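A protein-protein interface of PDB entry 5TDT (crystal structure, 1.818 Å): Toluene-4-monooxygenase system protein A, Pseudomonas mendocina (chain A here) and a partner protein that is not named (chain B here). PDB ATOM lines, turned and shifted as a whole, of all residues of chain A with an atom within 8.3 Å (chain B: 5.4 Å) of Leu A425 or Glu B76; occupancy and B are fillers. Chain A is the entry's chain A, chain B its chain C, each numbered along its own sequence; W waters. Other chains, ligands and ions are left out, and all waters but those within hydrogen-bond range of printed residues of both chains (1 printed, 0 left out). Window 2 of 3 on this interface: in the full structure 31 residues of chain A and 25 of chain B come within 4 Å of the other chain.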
ATOM      1  N   SER A 395      33.519  -4.722   9.064  1.00  0.00           N
ATOM      2  CA  SER A 395      32.406  -5.626   8.773  1.00  0.00           C
ATOM      3  C   SER A 395      31.086  -4.863   8.875  1.00  0.00           C
ATOM      4  O   SER A 395      30.909  -4.060   9.791  1.00  0.00           O
ATOM      5  CB  SER A 395      32.430  -6.800   9.748  1.00  0.00           C
ATOM      6  OG  SER A 395      33.752  -7.291   9.894  1.00  0.00           O
ATOM      7  N   VAL A 396      30.144  -5.140   7.953  1.00  0.00           N
ATOM      8  CA  VAL A 396      28.992  -4.268   7.707  1.00  0.00           C
ATOM      9  C   VAL A 396      27.675  -5.009   7.958  1.00  0.00           C
ATOM     10  O   VAL A 396      27.528  -6.180   7.591  1.00  0.00           O
ATOM     11  CB  VAL A 396      29.047  -3.698   6.267  1.00  0.00           C
ATOM     12  CG1 VAL A 396      27.809  -2.864   5.941  1.00  0.00           C
ATOM     13  CG2 VAL A 396      30.307  -2.849   6.081  1.00  0.00           C
ATOM     14  N   ASN A 398      23.989  -6.254   7.345  1.00  0.00           N
ATOM     15  CA  ASN A 398      23.213  -6.539   6.136  1.00  0.00           C
ATOM     16  C   ASN A 398      21.855  -5.849   6.114  1.00  0.00           C
ATOM     17  O   ASN A 398      21.110  -6.007   5.137  1.00  0.00           O
ATOM     18  CB  ASN A 398      23.021  -8.052   5.963  1.00  0.00           C
ATOM     19  CG  ASN A 398      24.194  -8.703   5.251  1.00  0.00           C
ATOM     20  OD1 ASN A 398      24.931  -9.483   5.847  1.00  0.00           O
ATOM     21  ND2 ASN A 398      24.379  -8.371   3.971  1.00  0.00           N
ATOM     22  N   VAL A 416      27.271  -9.539  17.318  1.00  0.00           N
ATOM     23  CA  VAL A 416      26.763  -9.617  15.950  1.00  0.00           C
ATOM     24  C   VAL A 416      25.625 -10.629  15.934  1.00  0.00           C
ATOM     25  O   VAL A 416      25.748 -11.711  16.516  1.00  0.00           O
ATOM     26  CB  VAL A 416      27.877 -10.043  14.975  1.00  0.00           C
ATOM     27  CG1 VAL A 416      27.328 -10.237  13.554  1.00  0.00           C
ATOM     28  CG2 VAL A 416      29.056  -9.044  15.027  1.00  0.00           C
ATOM     29  N   PHE A 417      24.521 -10.289  15.268  1.00  0.00           N
ATOM     30  CA  PHE A 417      23.345 -11.158  15.220  1.00  0.00           C
ATOM     31  C   PHE A 417      23.240 -11.734  13.817  1.00  0.00           C
ATOM     32  O   PHE A 417      22.940 -11.007  12.869  1.00  0.00           O
ATOM     33  CB  PHE A 417      22.095 -10.385  15.625  1.00  0.00           C
ATOM     34  CG  PHE A 417      22.188  -9.845  17.014  1.00  0.00           C
ATOM     35  CD1 PHE A 417      22.771  -8.607  17.244  1.00  0.00           C
ATOM     36  CD2 PHE A 417      21.783 -10.619  18.099  1.00  0.00           C
ATOM     37  CE1 PHE A 417      22.894  -8.102  18.553  1.00  0.00           C
ATOM     38  CE2 PHE A 417      21.914 -10.134  19.403  1.00  0.00           C
ATOM     39  CZ  PHE A 417      22.463  -8.873  19.627  1.00  0.00           C
ATOM     40  N   SER A 418      23.498 -13.032  13.687  1.00  0.00           N
ATOM     41  CA  SER A 418      23.691 -13.647  12.378  1.00  0.00           C
ATOM     42  C   SER A 418      22.536 -14.571  12.012  1.00  0.00           C
ATOM     43  O   SER A 418      21.683 -14.911  12.841  1.00  0.00           O
ATOM     44  CB  SER A 418      25.022 -14.401  12.346  1.00  0.00           C
ATOM     45  OG  SER A 418      26.089 -13.468  12.486  1.00  0.00           O
ATOM     46  N   LEU A 419      22.533 -14.983  10.741  1.00  0.00           N
ATOM     47  CA  LEU A 419      21.395 -15.693  10.152  1.00  0.00           C
ATOM     48  C   LEU A 419      21.832 -16.398   8.880  1.00  0.00           C
ATOM     49  O   LEU A 419      22.290 -15.750   7.933  1.00  0.00           O
ATOM     50  CB  LEU A 419      20.238 -14.728   9.844  1.00  0.00           C
ATOM     51  CG  LEU A 419      18.998 -15.417   9.233  1.00  0.00           C
ATOM     52  CD1 LEU A 419      18.298 -16.318  10.250  1.00  0.00           C
ATOM     53  CD2 LEU A 419      18.025 -14.390   8.677  1.00  0.00           C
ATOM     54  N   GLU A 420      21.667 -17.717   8.857  1.00  0.00           N
ATOM     55  CA  GLU A 420      21.783 -18.497   7.634  1.00  0.00           C
ATOM     56  C   GLU A 420      20.434 -18.476   6.933  1.00  0.00           C
ATOM     57  O   GLU A 420      19.414 -18.801   7.548  1.00  0.00           O
ATOM     58  CB  GLU A 420      22.189 -19.941   7.938  1.00  0.00           C
ATOM     59  CG  GLU A 420      23.610 -20.080   8.464  1.00  0.00           C
ATOM     60  CD  GLU A 420      24.022 -21.522   8.655  1.00  0.00           C
ATOM     61  OE1 GLU A 420      24.285 -22.221   7.643  1.00  0.00           O
ATOM     62  OE2 GLU A 420      24.052 -21.972   9.819  1.00  0.00           O
ATOM     63  N   HIS A 421      20.426 -18.121   5.648  1.00  0.00           N
ATOM     64  CA  HIS A 421      19.165 -18.033   4.909  1.00  0.00           C
ATOM     65  C   HIS A 421      19.443 -18.287   3.438  1.00  0.00           C
ATOM     66  O   HIS A 421      20.239 -17.560   2.838  1.00  0.00           O
ATOM     67  CB  HIS A 421      18.522 -16.659   5.109  1.00  0.00           C
ATOM     68  CG  HIS A 421      17.358 -16.376   4.202  1.00  0.00           C
ATOM     69  ND1 HIS A 421      16.110 -16.935   4.389  1.00  0.00           N
ATOM     70  CD2 HIS A 421      17.243 -15.558   3.126  1.00  0.00           C
ATOM     71  CE1 HIS A 421      15.284 -16.488   3.459  1.00  0.00           C
ATOM     72  NE2 HIS A 421      15.946 -15.652   2.677  1.00  0.00           N
ATOM     73  N   ASN A 422      18.799 -19.310   2.870  1.00  0.00           N
ATOM     74  CA  ASN A 422      18.923 -19.633   1.442  1.00  0.00           C
ATOM     75  C   ASN A 422      20.388 -19.738   1.011  1.00  0.00           C
ATOM     76  O   ASN A 422      20.824 -19.112   0.041  1.00  0.00           O
ATOM     77  CB  ASN A 422      18.181 -18.596   0.590  1.00  0.00           C
ATOM     78  CG  ASN A 422      16.669 -18.738   0.671  1.00  0.00           C
ATOM     79  OD1 ASN A 422      16.152 -19.745   1.145  1.00  0.00           O
ATOM     80  ND2 ASN A 422      15.956 -17.727   0.192  1.00  0.00           N
ATOM     81  N   GLY A 423      21.166 -20.500   1.776  1.00  0.00           N
ATOM     82  CA  GLY A 423      22.563 -20.732   1.438  1.00  0.00           C
ATOM     83  C   GLY A 423      23.472 -19.526   1.553  1.00  0.00           C
ATOM     84  O   GLY A 423      24.489 -19.451   0.854  1.00  0.00           O
ATOM     85  N   ARG A 424      23.136 -18.571   2.414  1.00  0.00           N
ATOM     86  CA  ARG A 424      23.951 -17.382   2.569  1.00  0.00           C
ATOM     87  C   ARG A 424      23.995 -16.999   4.040  1.00  0.00           C
ATOM     88  O   ARG A 424      22.998 -17.158   4.747  1.00  0.00           O
ATOM     89  CB  ARG A 424      23.379 -16.238   1.732  1.00  0.00           C
ATOM     90  CG  ARG A 424      24.236 -15.025   1.705  1.00  0.00           C
ATOM     91  CD  ARG A 424      23.750 -14.035   0.668  1.00  0.00           C
ATOM     92  NE  ARG A 424      24.188 -12.716   1.070  1.00  0.00           N
ATOM     93  CZ  ARG A 424      23.657 -11.583   0.645  1.00  0.00           C
ATOM     94  NH1 ARG A 424      22.650 -11.601  -0.217  1.00  0.00           N
ATOM     95  NH2 ARG A 424      24.139 -10.435   1.100  1.00  0.00           N
ATOM     96  N   LEU A 425      25.145 -16.493   4.496  1.00  0.00           N
ATOM     97  CA  LEU A 425      25.328 -16.062   5.881  1.00  0.00           C
ATOM     98  C   LEU A 425      25.227 -14.541   5.956  1.00  0.00           C
ATOM     99  O   LEU A 425      26.033 -13.835   5.341  1.00  0.00           O
ATOM    100  CB  LEU A 425      26.678 -16.533   6.434  1.00  0.00           C
ATOM    101  CG  LEU A 425      26.984 -16.162   7.897  1.00  0.00           C
ATOM    102  CD1 LEU A 425      25.856 -16.624   8.828  1.00  0.00           C
ATOM    103  CD2 LEU A 425      28.325 -16.760   8.365  1.00  0.00           C
ATOM    104  N   TYR A 426      24.235 -14.041   6.702  1.00  0.00           N
ATOM    105  CA  TYR A 426      24.038 -12.610   6.912  1.00  0.00           C
ATOM    106  C   TYR A 426      24.431 -12.259   8.339  1.00  0.00           C
ATOM    107  O   TYR A 426      24.316 -13.083   9.251  1.00  0.00           O
ATOM    108  CB  TYR A 426      22.578 -12.175   6.679  1.00  0.00           C
ATOM    109  CG  TYR A 426      21.968 -12.593   5.344  1.00  0.00           C
ATOM    110  CD1 TYR A 426      21.594 -13.909   5.113  1.00  0.00           C
ATOM    111  CD2 TYR A 426      21.728 -11.660   4.336  1.00  0.00           C
ATOM    112  CE1 TYR A 426      21.031 -14.296   3.904  1.00  0.00           C
ATOM    113  CE2 TYR A 426      21.159 -12.051   3.109  1.00  0.00           C
ATOM    114  CZ  TYR A 426      20.807 -13.362   2.917  1.00  0.00           C
ATOM    115  OH  TYR A 426      20.238 -13.770   1.722  1.00  0.00           O
ATOM    116  N   HIS A 427      24.903 -11.029   8.523  1.00  0.00           N
ATOM    117  CA  HIS A 427      25.287 -10.526   9.833  1.00  0.00           C
ATOM    118  C   HIS A 427      24.567  -9.211  10.086  1.00  0.00           C
ATOM    119  O   HIS A 427      24.521  -8.343   9.206  1.00  0.00           O
ATOM    120  CB  HIS A 427      26.810 -10.309   9.934  1.00  0.00           C
ATOM    121  CG  HIS A 427      27.619 -11.547   9.681  1.00  0.00           C
ATOM    122  ND1 HIS A 427      27.549 -12.658  10.493  1.00  0.00           N
ATOM    123  CD2 HIS A 427      28.523 -11.842   8.712  1.00  0.00           C
ATOM    124  CE1 HIS A 427      28.379 -13.584  10.041  1.00  0.00           C
ATOM    125  NE2 HIS A 427      28.983 -13.113   8.962  1.00  0.00           N
ATOM    126  N   PHE A 428      24.026  -9.054  11.290  1.00  0.00           N
ATOM    127  CA  PHE A 428      23.256  -7.860  11.623  1.00  0.00           C
ATOM    128  C   PHE A 428      23.798  -7.209  12.885  1.00  0.00           C
ATOM    129  O   PHE A 428      24.334  -7.880  13.773  1.00  0.00           O
ATOM    130  CB  PHE A 428      21.768  -8.180  11.795  1.00  0.00           C
ATOM    131  CG  PHE A 428      21.143  -8.758  10.553  1.00  0.00           C
ATOM    132  CD1 PHE A 428      20.785  -7.928   9.493  1.00  0.00           C
ATOM    133  CD2 PHE A 428      20.935 -10.131  10.437  1.00  0.00           C
ATOM    134  CE1 PHE A 428      20.224  -8.452   8.334  1.00  0.00           C
ATOM    135  CE2 PHE A 428      20.379 -10.672   9.276  1.00  0.00           C
ATOM    136  CZ  PHE A 428      20.023  -9.824   8.223  1.00  0.00           C
ATOM    137  N   PHE A 437      14.745  -7.726   8.859  1.00  0.00           N
ATOM    138  CA  PHE A 437      14.979  -8.657   7.749  1.00  0.00           C
ATOM    139  C   PHE A 437      13.913  -9.745   7.710  1.00  0.00           C
ATOM    140  O   PHE A 437      13.327 -10.028   6.655  1.00  0.00           O
ATOM    141  CB  PHE A 437      16.370  -9.285   7.893  1.00  0.00           C
ATOM    142  CG  PHE A 437      16.780 -10.163   6.734  1.00  0.00           C
ATOM    143  CD1 PHE A 437      16.439 -11.510   6.701  1.00  0.00           C
ATOM    144  CD2 PHE A 437      17.530  -9.649   5.699  1.00  0.00           C
ATOM    145  CE1 PHE A 437      16.825 -12.325   5.649  1.00  0.00           C
ATOM    146  CE2 PHE A 437      17.929 -10.462   4.632  1.00  0.00           C
ATOM    147  CZ  PHE A 437      17.580 -11.796   4.614  1.00  0.00           C
ATOM    148  N   ASN A 449      25.673  -6.220   0.676  1.00  0.00           N
ATOM    149  CA  ASN A 449      26.273  -4.994   1.175  1.00  0.00           C
ATOM    150  C   ASN A 449      27.669  -4.822   0.574  1.00  0.00           C
ATOM    151  O   ASN A 449      28.195  -5.707  -0.107  1.00  0.00           O
ATOM    152  CB  ASN A 449      26.264  -4.946   2.717  1.00  0.00           C
ATOM    153  CG  ASN A 449      27.319  -5.835   3.391  1.00  0.00           C
ATOM    154  OD1 ASN A 449      28.431  -6.019   2.899  1.00  0.00           O
ATOM    155  ND2 ASN A 449      26.967  -6.347   4.582  1.00  0.00           N
ATOM    156  N   ASP A 452      30.088  -7.507   1.150  1.00  0.00           N
ATOM    157  CA  ASP A 452      29.691  -8.683   0.373  1.00  0.00           C
ATOM    158  C   ASP A 452      30.193  -8.581  -1.063  1.00  0.00           C
ATOM    159  O   ASP A 452      30.679  -9.564  -1.637  1.00  0.00           O
ATOM    160  CB  ASP A 452      28.167  -8.838   0.364  1.00  0.00           C
ATOM    161  CG  ASP A 452      27.580  -9.067   1.744  1.00  0.00           C
ATOM    162  OD1 ASP A 452      28.226  -9.732   2.578  1.00  0.00           O
ATOM    163  OD2 ASP A 452      26.447  -8.592   1.983  1.00  0.00           O
ATOM    164  N   LEU A 455      34.026  -9.041  -1.275  1.00  0.00           N
ATOM    165  CA  LEU A 455      34.412 -10.441  -1.165  1.00  0.00           C
ATOM    166  C   LEU A 455      33.957 -11.281  -2.353  1.00  0.00           C
ATOM    167  O   LEU A 455      34.491 -12.380  -2.558  1.00  0.00           O
ATOM    168  CB  LEU A 455      33.848 -11.034   0.125  1.00  0.00           C
ATOM    169  CG  LEU A 455      34.527 -10.571   1.419  1.00  0.00           C
ATOM    170  CD1 LEU A 455      33.791 -11.085   2.650  1.00  0.00           C
ATOM    171  CD2 LEU A 455      35.956 -11.056   1.417  1.00  0.00           C
ATOM    172  N   PRO B   5      38.454 -15.561   4.355  1.00  0.00           N
ATOM    173  CA  PRO B   5      37.984 -14.348   5.035  1.00  0.00           C
ATOM    174  C   PRO B   5      37.201 -14.691   6.292  1.00  0.00           C
ATOM    175  O   PRO B   5      36.363 -15.601   6.296  1.00  0.00           O
ATOM    176  CB  PRO B   5      37.079 -13.688   3.984  1.00  0.00           C
ATOM    177  CG  PRO B   5      36.503 -14.856   3.244  1.00  0.00           C
ATOM    178  CD  PRO B   5      37.631 -15.875   3.169  1.00  0.00           C
ATOM    179  N   VAL B   6      37.493 -13.961   7.372  1.00  0.00           N
ATOM    180  CA  VAL B   6      36.692 -14.002   8.591  1.00  0.00           C
ATOM    181  C   VAL B   6      36.353 -12.570   8.992  1.00  0.00           C
ATOM    182  O   VAL B   6      36.971 -11.607   8.535  1.00  0.00           O
ATOM    183  CB  VAL B   6      37.394 -14.730   9.766  1.00  0.00           C
ATOM    184  CG1 VAL B   6      37.672 -16.192   9.430  1.00  0.00           C
ATOM    185  CG2 VAL B   6      38.689 -14.021  10.157  1.00  0.00           C
ATOM    186  N   HIS B   7      35.349 -12.443   9.857  1.00  0.00           N
ATOM    187  CA  HIS B   7      35.026 -11.187  10.524  1.00  0.00           C
ATOM    188  C   HIS B   7      35.437 -11.316  11.986  1.00  0.00           C
ATOM    189  O   HIS B   7      34.948 -12.198  12.692  1.00  0.00           O
ATOM    190  CB  HIS B   7      33.537 -10.869  10.380  1.00  0.00           C
ATOM    191  CG  HIS B   7      33.101 -10.707   8.960  1.00  0.00           C
ATOM    192  ND1 HIS B   7      33.409  -9.590   8.213  1.00  0.00           N
ATOM    193  CD2 HIS B   7      32.412 -11.533   8.136  1.00  0.00           C
ATOM    194  CE1 HIS B   7      32.918  -9.729   6.994  1.00  0.00           C
ATOM    195  NE2 HIS B   7      32.313 -10.901   6.920  1.00  0.00           N
ATOM    196  N   LYS B  54      34.993 -18.872  18.376  1.00  0.00           N
ATOM    197  CA  LYS B  54      33.808 -18.450  17.630  1.00  0.00           C
ATOM    198  C   LYS B  54      33.112 -17.308  18.379  1.00  0.00           C
ATOM    199  O   LYS B  54      33.193 -17.219  19.606  1.00  0.00           O
ATOM    200  CB  LYS B  54      32.837 -19.616  17.443  1.00  0.00           C
ATOM    201  CG  LYS B  54      33.272 -20.652  16.428  1.00  0.00           C
ATOM    202  CD  LYS B  54      32.125 -21.616  16.110  1.00  0.00           C
ATOM    203  CE  LYS B  54      30.955 -20.892  15.450  1.00  0.00           C
ATOM    204  NZ  LYS B  54      31.205 -20.554  14.017  1.00  0.00           N
ATOM    205  N   GLY B  71      36.801 -26.301  11.543  1.00  0.00           N
ATOM    206  CA  GLY B  71      35.427 -26.345  11.098  1.00  0.00           C
ATOM    207  C   GLY B  71      34.781 -24.989  10.895  1.00  0.00           C
ATOM    208  O   GLY B  71      33.581 -24.935  10.600  1.00  0.00           O
ATOM    209  N   LEU B  72      35.531 -23.893  11.049  1.00  0.00           N
ATOM    210  CA  LEU B  72      35.009 -22.568  10.723  1.00  0.00           C
ATOM    211  C   LEU B  72      34.702 -22.474   9.236  1.00  0.00           C
ATOM    212  O   LEU B  72      35.422 -23.032   8.403  1.00  0.00           O
ATOM    213  CB  LEU B  72      36.025 -21.482  11.096  1.00  0.00           C
ATOM    214  CG  LEU B  72      36.183 -21.044  12.550  1.00  0.00           C
ATOM    215  CD1 LEU B  72      37.432 -20.150  12.689  1.00  0.00           C
ATOM    216  CD2 LEU B  72      34.939 -20.305  13.015  1.00  0.00           C
ATOM    217  N   ASN B  73      33.622 -21.752   8.901  1.00  0.00           N
ATOM    218  CA  ASN B  73      33.311 -21.464   7.508  1.00  0.00           C
ATOM    219  C   ASN B  73      33.707 -20.033   7.169  1.00  0.00           C
ATOM    220  O   ASN B  73      33.695 -19.157   8.043  1.00  0.00           O
ATOM    221  CB  ASN B  73      31.818 -21.645   7.223  1.00  0.00           C
ATOM    222  CG  ASN B  73      31.334 -23.046   7.510  1.00  0.00           C
ATOM    223  OD1 ASN B  73      31.704 -23.994   6.817  1.00  0.00           O
ATOM    224  ND2 ASN B  73      30.492 -23.186   8.527  1.00  0.00           N
ATOM    225  N   PRO B  74      34.050 -19.762   5.909  1.00  0.00           N
ATOM    226  CA  PRO B  74      34.399 -18.391   5.524  1.00  0.00           C
ATOM    227  C   PRO B  74      33.295 -17.414   5.900  1.00  0.00           C
ATOM    228  O   PRO B  74      32.102 -17.725   5.817  1.00  0.00           O
ATOM    229  CB  PRO B  74      34.583 -18.487   4.004  1.00  0.00           C
ATOM    230  CG  PRO B  74      34.997 -19.907   3.779  1.00  0.00           C
ATOM    231  CD  PRO B  74      34.166 -20.693   4.774  1.00  0.00           C
ATOM    232  N   THR B  75      33.720 -16.228   6.339  1.00  0.00           N
ATOM    233  CA  THR B  75      32.892 -15.085   6.722  1.00  0.00           C
ATOM    234  C   THR B  75      32.144 -15.306   8.030  1.00  0.00           C
ATOM    235  O   THR B  75      31.311 -14.483   8.382  1.00  0.00           O
ATOM    236  CB  THR B  75      31.897 -14.677   5.621  1.00  0.00           C
ATOM    237  OG1 THR B  75      30.868 -15.672   5.487  1.00  0.00           O
ATOM    238  CG2 THR B  75      32.624 -14.514   4.275  1.00  0.00           C
ATOM    239  N   GLU B  76      32.437 -16.372   8.773  1.00  0.00           N
ATOM    240  CA  GLU B  76      31.936 -16.465  10.142  1.00  0.00           C
ATOM    241  C   GLU B  76      32.670 -15.455  11.037  1.00  0.00           C
ATOM    242  O   GLU B  76      33.771 -14.987  10.722  1.00  0.00           O
ATOM    243  CB  GLU B  76      32.095 -17.903  10.669  1.00  0.00           C
ATOM    244  CG  GLU B  76      31.032 -18.871  10.080  1.00  0.00           C
ATOM    245  CD  GLU B  76      31.109 -20.301  10.626  1.00  0.00           C
ATOM    246  OE1 GLU B  76      32.168 -20.707  11.143  1.00  0.00           O
ATOM    247  OE2 GLU B  76      30.094 -21.028  10.526  1.00  0.00           O
ATOM    248  N   VAL B  77      32.047 -15.110  12.166  1.00  0.00           N
ATOM    249  CA  VAL B  77      32.601 -14.111  13.084  1.00  0.00           C
ATOM    250  C   VAL B  77      33.417 -14.825  14.157  1.00  0.00           C
ATOM    251  O   VAL B  77      32.970 -15.834  14.719  1.00  0.00           O
ATOM    252  CB  VAL B  77      31.485 -13.273  13.732  1.00  0.00           C
ATOM    253  CG1 VAL B  77      32.077 -12.208  14.677  1.00  0.00           C
ATOM    254  CG2 VAL B  77      30.581 -12.652  12.678  1.00  0.00           C
ATOM    255  N   ILE B  78      34.611 -14.301  14.460  1.00  0.00           N
ATOM    256  CA  ILE B  78      35.422 -14.824  15.553  1.00  0.00           C
ATOM    257  C   ILE B  78      35.759 -13.680  16.497  1.00  0.00           C
ATOM    258  O   ILE B  78      35.700 -12.503  16.131  1.00  0.00           O
ATOM    259  CB  ILE B  78      36.727 -15.512  15.076  1.00  0.00           C
ATOM    260  CG1 ILE B  78      37.631 -14.510  14.360  1.00  0.00           C
ATOM    261  CG2 ILE B  78      36.415 -16.764  14.237  1.00  0.00           C
ATOM    262  CD1 ILE B  78      39.038 -15.098  13.905  1.00  0.00           C
HETATM  263  O   HOH W   1      28.689 -13.489   5.756  1.00  0.00           O
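Hydrophobic or aromatic side chains of chain B that line the printed part of chain A: Pro B5, His B7 and Val B77.
Among the printed residues, 8 pairs touch across the chains.
Among the printed residues, no Asp or Glu carboxylate lies within 4 Å of a Lys or Arg side-chain nitrogen of the other chain.
Among the printed residues, pairs that only touch across the chains: Leu A425 with Thr B75 (3.8 Å), Leu A425 with Glu B76 (3.8 Å), His A427 with His B7 (3.9 Å), His A427 with Val B77 (3.6 Å), Leu A455 with Pro B5 (3.8 Å) and Leu A455 with Thr B75 (3.97 Å).
The backbone NH of Asn A398 lies within hydrogen-bond range of the backbone carbonyl oxygen of His A427, at 2.8 Å.
OG of Ser A418 is in hydrogen-bond range of ND1 of His A427 (2.6 Å).
The backbone carbonyl oxygen (O) of Pro B5 is in hydrogen-bond range of the backbone NH (N) of Thr B75.
N of His B7 lies within hydrogen-bond range of O of Glu B76, at 3.1 Å.
The backbone carbonyl oxygen (O) of His B7 is in hydrogen-bond range of the backbone NH (N) of Ile B78 (2.8 Å).
The backbone NH (N) of Asn B73 is in hydrogen-bond range of the side-chain carboxylate (OE1) of Glu B76, 2.9 Å away.
OG of Ser A395 sits at hydrogen-bond distance from ND1 of His B7 (2.9 Å).
A ring nitrogen (NE2) of His A427 is in hydrogen-bond range of the backbone carbonyl oxygen (O) of Thr B75 (2.8 Å).
Leu A425 touches just these residues of chain B: Thr B75 (3.8 Å) and Glu B76 (3.8 Å).
Printed residues of chain A within 4 Å of Glu B76: Leu A425.
Printed residues of chain A within 4 Å of Thr B75: Leu A425, His A427 and Leu A455.
Printed residues of chain B within 4 Å of Leu A455: Pro B5 (3.8 Å) and Thr B75 (3.97 Å).
Of the printed residues of chain A, Pro B5 touches Leu A455 (3.8 Å).
Of the printed residues of chain A, His B7 touches Ser A395 (2.9 Å) and His A427 (3.9 Å).
Printed residues of chain A within 4 Å of Val B77: His A427 (3.6 Å).
The nearest printed residue of chain B that does not touch Ser A395 is Val B6 (5.6 Å).
Water W1 lies within hydrogen-bond range of the backbone carbonyl oxygen (O) of Leu A425, the side-chain hydroxyl (OG1) of Thr B75 and a ring nitrogen (NE2) of His A427.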
